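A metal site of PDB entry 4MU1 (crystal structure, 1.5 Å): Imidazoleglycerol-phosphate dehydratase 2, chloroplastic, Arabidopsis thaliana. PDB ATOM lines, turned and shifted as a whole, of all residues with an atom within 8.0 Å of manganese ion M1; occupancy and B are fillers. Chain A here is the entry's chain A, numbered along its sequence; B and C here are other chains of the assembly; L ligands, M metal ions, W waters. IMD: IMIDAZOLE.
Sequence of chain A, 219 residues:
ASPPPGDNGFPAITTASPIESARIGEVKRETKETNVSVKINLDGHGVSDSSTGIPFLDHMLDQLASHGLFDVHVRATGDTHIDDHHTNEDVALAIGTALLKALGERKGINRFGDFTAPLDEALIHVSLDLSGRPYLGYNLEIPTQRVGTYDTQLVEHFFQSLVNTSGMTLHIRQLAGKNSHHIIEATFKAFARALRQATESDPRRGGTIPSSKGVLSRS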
ATOM      1  N   HIS A  85      -8.807  -4.511   5.185  1.00  0.00           N
ATOM      2  CA  HIS A  85      -9.711  -5.356   4.373  1.00  0.00           C
ATOM      3  C   HIS A  85      -9.041  -5.956   3.143  1.00  0.00           C
ATOM      4  O   HIS A  85      -9.118  -7.186   2.923  1.00  0.00           O
ATOM      5  CB  HIS A  85     -10.912  -4.524   3.927  1.00  0.00           C
ATOM      6  CG  HIS A  85     -12.007  -5.323   3.288  1.00  0.00           C
ATOM      7  ND1 HIS A  85     -13.278  -5.453   3.826  1.00  0.00           N
ATOM      8  CD2 HIS A  85     -12.038  -5.992   2.101  1.00  0.00           C
ATOM      9  CE1 HIS A  85     -14.035  -6.172   3.008  1.00  0.00           C
ATOM     10  NE2 HIS A  85     -13.313  -6.507   1.947  1.00  0.00           N
ATOM     11  N   HIS A  86      -8.413  -5.114   2.325  1.00  0.00           N
ATOM     12  CA  HIS A  86      -7.906  -5.637   1.069  1.00  0.00           C
ATOM     13  C   HIS A  86      -6.752  -6.627   1.289  1.00  0.00           C
ATOM     14  O   HIS A  86      -6.644  -7.638   0.613  1.00  0.00           O
ATOM     15  CB  HIS A  86      -7.499  -4.543   0.069  1.00  0.00           C
ATOM     16  CG  HIS A  86      -8.541  -3.507  -0.214  1.00  0.00           C
ATOM     17  ND1 HIS A  86      -8.212  -2.231  -0.613  1.00  0.00           N
ATOM     18  CD2 HIS A  86      -9.889  -3.581  -0.249  1.00  0.00           C
ATOM     19  CE1 HIS A  86      -9.321  -1.543  -0.836  1.00  0.00           C
ATOM     20  NE2 HIS A  86     -10.359  -2.347  -0.612  1.00  0.00           N
ATOM     21  N   ASN A  88      -6.187  -8.472   4.047  1.00  0.00           N
ATOM     22  CA  ASN A  88      -6.796  -9.682   4.646  1.00  0.00           C
ATOM     23  C   ASN A  88      -7.398 -10.598   3.565  1.00  0.00           C
ATOM     24  O   ASN A  88      -7.131 -11.797   3.523  1.00  0.00           O
ATOM     25  CB  ASN A  88      -7.849  -9.239   5.639  1.00  0.00           C
ATOM     26  CG  ASN A  88      -8.493 -10.376   6.431  1.00  0.00           C
ATOM     27  OD1 ASN A  88      -7.951 -10.883   7.419  1.00  0.00           O
ATOM     28  ND2 ASN A  88      -9.686 -10.730   6.033  1.00  0.00           N
ATOM     29  N   GLU A  89      -8.141  -9.980   2.648  1.00  0.00           N
ATOM     30  CA  GLU A  89      -8.833 -10.683   1.557  1.00  0.00           C
ATOM     31  C   GLU A  89      -7.794 -11.327   0.618  1.00  0.00           C
ATOM     32  O   GLU A  89      -7.891 -12.519   0.239  1.00  0.00           O
ATOM     33  CB  GLU A  89      -9.711  -9.716   0.773  1.00  0.00           C
ATOM     34  CG  GLU A  89     -10.421 -10.377  -0.390  1.00  0.00           C
ATOM     35  CD  GLU A  89     -11.633  -9.607  -0.904  1.00  0.00           C
ATOM     36  OE1 GLU A  89     -11.971  -8.570  -0.259  1.00  0.00           O
ATOM     37  OE2 GLU A  89     -12.269 -10.136  -1.870  1.00  0.00           O
ATOM     38  N   ASP A  90      -6.794 -10.533   0.220  1.00  0.00           N
ATOM     39  CA  ASP A  90      -5.894 -11.016  -0.809  1.00  0.00           C
ATOM     40  C   ASP A  90      -4.923 -12.108  -0.249  1.00  0.00           C
ATOM     41  O   ASP A  90      -4.510 -13.045  -0.937  1.00  0.00           O
ATOM     42  CB  ASP A  90      -5.151  -9.843  -1.453  1.00  0.00           C
ATOM     43  CG  ASP A  90      -6.015  -9.051  -2.455  1.00  0.00           C
ATOM     44  OD1 ASP A  90      -7.061  -9.561  -2.895  1.00  0.00           O
ATOM     45  OD2 ASP A  90      -5.627  -7.879  -2.730  1.00  0.00           O
ATOM     46  N   LEU A  93      -7.245 -15.251  -0.197  1.00  0.00           N
ATOM     47  CA  LEU A  93      -7.443 -15.761  -1.576  1.00  0.00           C
ATOM     48  C   LEU A  93      -6.180 -16.563  -1.936  1.00  0.00           C
ATOM     49  O   LEU A  93      -6.261 -17.654  -2.506  1.00  0.00           O
ATOM     50  CB  LEU A  93      -7.710 -14.630  -2.588  1.00  0.00           C
ATOM     51  CG  LEU A  93      -9.042 -13.908  -2.415  1.00  0.00           C
ATOM     52  CD1 LEU A  93      -9.063 -12.705  -3.292  1.00  0.00           C
ATOM     53  CD2 LEU A  93     -10.182 -14.836  -2.780  1.00  0.00           C
ATOM     54  N   LEU A 154     -13.339  -9.145   9.802  1.00  0.00           N
ATOM     55  CA  LEU A 154     -12.415  -9.731   8.818  1.00  0.00           C
ATOM     56  C   LEU A 154     -12.184 -11.230   8.993  1.00  0.00           C
ATOM     57  O   LEU A 154     -11.668 -11.875   8.088  1.00  0.00           O
ATOM     58  CB  LEU A 154     -11.097  -8.957   8.839  1.00  0.00           C
ATOM     59  CG  LEU A 154     -11.297  -7.499   8.445  1.00  0.00           C
ATOM     60  CD1 LEU A 154      -9.976  -6.738   8.514  1.00  0.00           C
ATOM     61  CD2 LEU A 154     -11.912  -7.355   7.032  1.00  0.00           C
ATOM     62  N   HIS A 157     -14.476 -12.961   6.561  1.00  0.00           N
ATOM     63  CA  HIS A 157     -14.012 -12.695   5.220  1.00  0.00           C
ATOM     64  C   HIS A 157     -12.769 -13.491   4.879  1.00  0.00           C
ATOM     65  O   HIS A 157     -12.608 -13.952   3.741  1.00  0.00           O
ATOM     66  CB  HIS A 157     -13.744 -11.183   5.024  1.00  0.00           C
ATOM     67  CG  HIS A 157     -13.806 -10.728   3.594  1.00  0.00           C
ATOM     68  ND1 HIS A 157     -13.381 -11.495   2.532  1.00  0.00           N
ATOM     69  CD2 HIS A 157     -14.257  -9.570   3.063  1.00  0.00           C
ATOM     70  CE1 HIS A 157     -13.558 -10.808   1.418  1.00  0.00           C
ATOM     71  NE2 HIS A 157     -14.099  -9.654   1.707  1.00  0.00           N
ATOM     72  N   SER A 161     -12.989 -16.100   1.685  1.00  0.00           N
ATOM     73  CA  SER A 161     -12.082 -15.929   0.579  1.00  0.00           C
ATOM     74  C   SER A 161     -11.218 -17.207   0.395  1.00  0.00           C
ATOM     75  O   SER A 161     -11.016 -17.675  -0.708  1.00  0.00           O
ATOM     76  CB  SER A 161     -11.196 -14.721   0.814  1.00  0.00           C
ATOM     77  OG  SER A 161     -11.966 -13.531   0.733  1.00  0.00           O
ATOM     78  N   LEU B 119     -21.813  -5.723  -3.948  1.00  0.00           N
ATOM     79  CA  LEU B 119     -20.414  -6.003  -3.631  1.00  0.00           C
ATOM     80  C   LEU B 119     -20.473  -7.197  -2.695  1.00  0.00           C
ATOM     81  O   LEU B 119     -20.845  -7.078  -1.503  1.00  0.00           O
ATOM     82  CB  LEU B 119     -19.682  -4.817  -3.027  1.00  0.00           C
ATOM     83  CG  LEU B 119     -18.159  -4.918  -3.041  1.00  0.00           C
ATOM     84  CD1 LEU B 119     -17.523  -3.718  -2.344  1.00  0.00           C
ATOM     85  CD2 LEU B 119     -17.537  -6.209  -2.605  1.00  0.00           C
ATOM     86  N   ASP B 120     -20.175  -8.373  -3.248  1.00  0.00           N
ATOM     87  CA  ASP B 120     -20.364  -9.621  -2.549  1.00  0.00           C
ATOM     88  C   ASP B 120     -21.767  -9.684  -1.950  1.00  0.00           C
ATOM     89  O   ASP B 120     -22.739  -9.592  -2.686  1.00  0.00           O
ATOM     90  CB  ASP B 120     -19.253  -9.866  -1.527  1.00  0.00           C
ATOM     91  CG  ASP B 120     -17.893 -10.144  -2.158  1.00  0.00           C
ATOM     92  OD1 ASP B 120     -17.787 -10.155  -3.410  1.00  0.00           O
ATOM     93  OD2 ASP B 120     -16.944 -10.411  -1.365  1.00  0.00           O
ATOM     94  N   GLU B 121     -21.885  -9.845  -0.628  1.00  0.00           N
ATOM     95  CA  GLU B 121     -23.185  -9.992   0.009  1.00  0.00           C
ATOM     96  C   GLU B 121     -24.000  -8.709   0.118  1.00  0.00           C
ATOM     97  O   GLU B 121     -25.194  -8.731   0.454  1.00  0.00           O
ATOM     98  CB  GLU B 121     -22.990 -10.628   1.391  1.00  0.00           C
ATOM     99  CG  GLU B 121     -22.765  -9.690   2.580  1.00  0.00           C
ATOM    100  CD  GLU B 121     -21.548  -8.783   2.486  1.00  0.00           C
ATOM    101  OE1 GLU B 121     -20.573  -9.118   1.821  1.00  0.00           O
ATOM    102  OE2 GLU B 121     -21.606  -7.714   3.199  1.00  0.00           O
ATOM    103  N   ASN B 179     -20.879  -6.744   5.828  1.00  0.00           N
ATOM    104  CA  ASN B 179     -19.569  -6.167   6.002  1.00  0.00           C
ATOM    105  C   ASN B 179     -19.636  -4.654   5.745  1.00  0.00           C
ATOM    106  O   ASN B 179     -20.120  -4.247   4.701  1.00  0.00           O
ATOM    107  CB  ASN B 179     -18.551  -6.866   5.078  1.00  0.00           C
ATOM    108  CG  ASN B 179     -17.170  -6.249   5.189  1.00  0.00           C
ATOM    109  OD1 ASN B 179     -16.886  -5.169   4.683  1.00  0.00           O
ATOM    110  ND2 ASN B 179     -16.300  -6.971   5.820  1.00  0.00           N
ATOM    111  N   HIS B 181     -17.386  -2.275   5.122  1.00  0.00           N
ATOM    112  CA  HIS B 181     -16.647  -1.808   3.921  1.00  0.00           C
ATOM    113  C   HIS B 181     -17.447  -2.147   2.662  1.00  0.00           C
ATOM    114  O   HIS B 181     -17.589  -1.300   1.770  1.00  0.00           O
ATOM    115  CB  HIS B 181     -15.229  -2.408   3.993  1.00  0.00           C
ATOM    116  CG  HIS B 181     -14.262  -1.985   2.952  1.00  0.00           C
ATOM    117  ND1 HIS B 181     -12.938  -1.752   3.293  1.00  0.00           N
ATOM    118  CD2 HIS B 181     -14.335  -1.847   1.602  1.00  0.00           C
ATOM    119  CE1 HIS B 181     -12.241  -1.472   2.195  1.00  0.00           C
ATOM    120  NE2 HIS B 181     -13.068  -1.477   1.169  1.00  0.00           N
ATOM    121  N   HIS B 182     -17.975  -3.352   2.565  1.00  0.00           N
ATOM    122  CA  HIS B 182     -18.769  -3.754   1.395  1.00  0.00           C
ATOM    123  C   HIS B 182     -19.992  -2.866   1.246  1.00  0.00           C
ATOM    124  O   HIS B 182     -20.341  -2.448   0.133  1.00  0.00           O
ATOM    125  CB  HIS B 182     -19.225  -5.204   1.445  1.00  0.00           C
ATOM    126  CG  HIS B 182     -18.104  -6.197   1.296  1.00  0.00           C
ATOM    127  ND1 HIS B 182     -18.281  -7.566   1.440  1.00  0.00           N
ATOM    128  CD2 HIS B 182     -16.793  -6.034   0.990  1.00  0.00           C
ATOM    129  CE1 HIS B 182     -17.148  -8.182   1.215  1.00  0.00           C
ATOM    130  NE2 HIS B 182     -16.228  -7.288   0.934  1.00  0.00           N
ATOM    131  N   GLU B 185     -18.844   0.750   0.166  1.00  0.00           N
ATOM    132  CA  GLU B 185     -18.285   0.724  -1.180  1.00  0.00           C
ATOM    133  C   GLU B 185     -19.332   0.441  -2.254  1.00  0.00           C
ATOM    134  O   GLU B 185     -19.368   1.092  -3.312  1.00  0.00           O
ATOM    135  CB  GLU B 185     -17.094  -0.217  -1.260  1.00  0.00           C
ATOM    136  CG  GLU B 185     -16.308  -0.074  -2.560  1.00  0.00           C
ATOM    137  CD  GLU B 185     -15.045  -0.906  -2.553  1.00  0.00           C
ATOM    138  OE1 GLU B 185     -14.336  -0.946  -1.492  1.00  0.00           O
ATOM    139  OE2 GLU B 185     -14.776  -1.567  -3.612  1.00  0.00           O
ATOM    140  N   ARG C 133     -15.574 -12.973  -7.976  1.00  0.00           N
ATOM    141  CA  ARG C 133     -15.774 -13.555  -6.640  1.00  0.00           C
ATOM    142  C   ARG C 133     -17.182 -14.155  -6.564  1.00  0.00           C
ATOM    143  O   ARG C 133     -18.185 -13.419  -6.761  1.00  0.00           O
ATOM    144  CB  ARG C 133     -15.711 -12.472  -5.582  1.00  0.00           C
ATOM    145  CG  ARG C 133     -14.384 -11.743  -5.487  1.00  0.00           C
ATOM    146  CD  ARG C 133     -14.390 -10.702  -4.352  1.00  0.00           C
ATOM    147  NE  ARG C 133     -15.314  -9.638  -4.708  1.00  0.00           N
ATOM    148  CZ  ARG C 133     -15.032  -8.549  -5.386  1.00  0.00           C
ATOM    149  NH1 ARG C 133     -13.779  -8.320  -5.762  1.00  0.00           N
ATOM    150  NH2 ARG C 133     -15.984  -7.694  -5.722  1.00  0.00           N
HETATM  151  N1  IMD L   1     -13.880  -4.221  -2.110  1.00  0.00           N
HETATM  152  C2  IMD L   1     -13.866  -4.826  -0.898  1.00  0.00           C
HETATM  153  N3  IMD L   1     -13.804  -6.138  -1.167  1.00  0.00           N
HETATM  154  C4  IMD L   1     -13.753  -6.366  -2.511  1.00  0.00           C
HETATM  155  C5  IMD L   1     -13.832  -5.127  -3.091  1.00  0.00           C
HETATM  156 MN    MN M   1     -14.060  -7.811   0.288  1.00  0.00          MN
HETATM  157 MN    MN M   2     -12.352  -1.254  -0.913  1.00  0.00          MN
HETATM  158  O   HOH W   1     -14.693  -9.050  -1.448  1.00  0.00           O
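The side-chain hydroxyl (OG) of Ser 161 is in hydrogen-bond range of a ring nitrogen (ND1) of His 157 (3.1 Å). The side-chain carboxylate (OE1) of Glu 121 of chain B lies within hydrogen-bond range of a ring nitrogen (ND1) of His 182 of chain B, at 2.8 Å. OD1 of Asn 179 of chain B sits at hydrogen-bond distance from N of His 182 of chain B.
Four residues have an atom within 4 Å of manganese ion M1: His 85, Glu 89, His 157 and His 182 of chain B.
Manganese ion M1 is bound by water W1, a nitrogen (N3) of the ligand, a ring nitrogen (NE2) of His 85, the side-chain carboxylate (OE1) of Glu 89, a ring nitrogen (NE2) of His 182 of chain B and a ring nitrogen (NE2) of His 157.
Water W1 lies within hydrogen-bond range of OD2 of Asp 120 of chain B, OE2 of Glu 89 and NE of Arg 133 of chain C.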
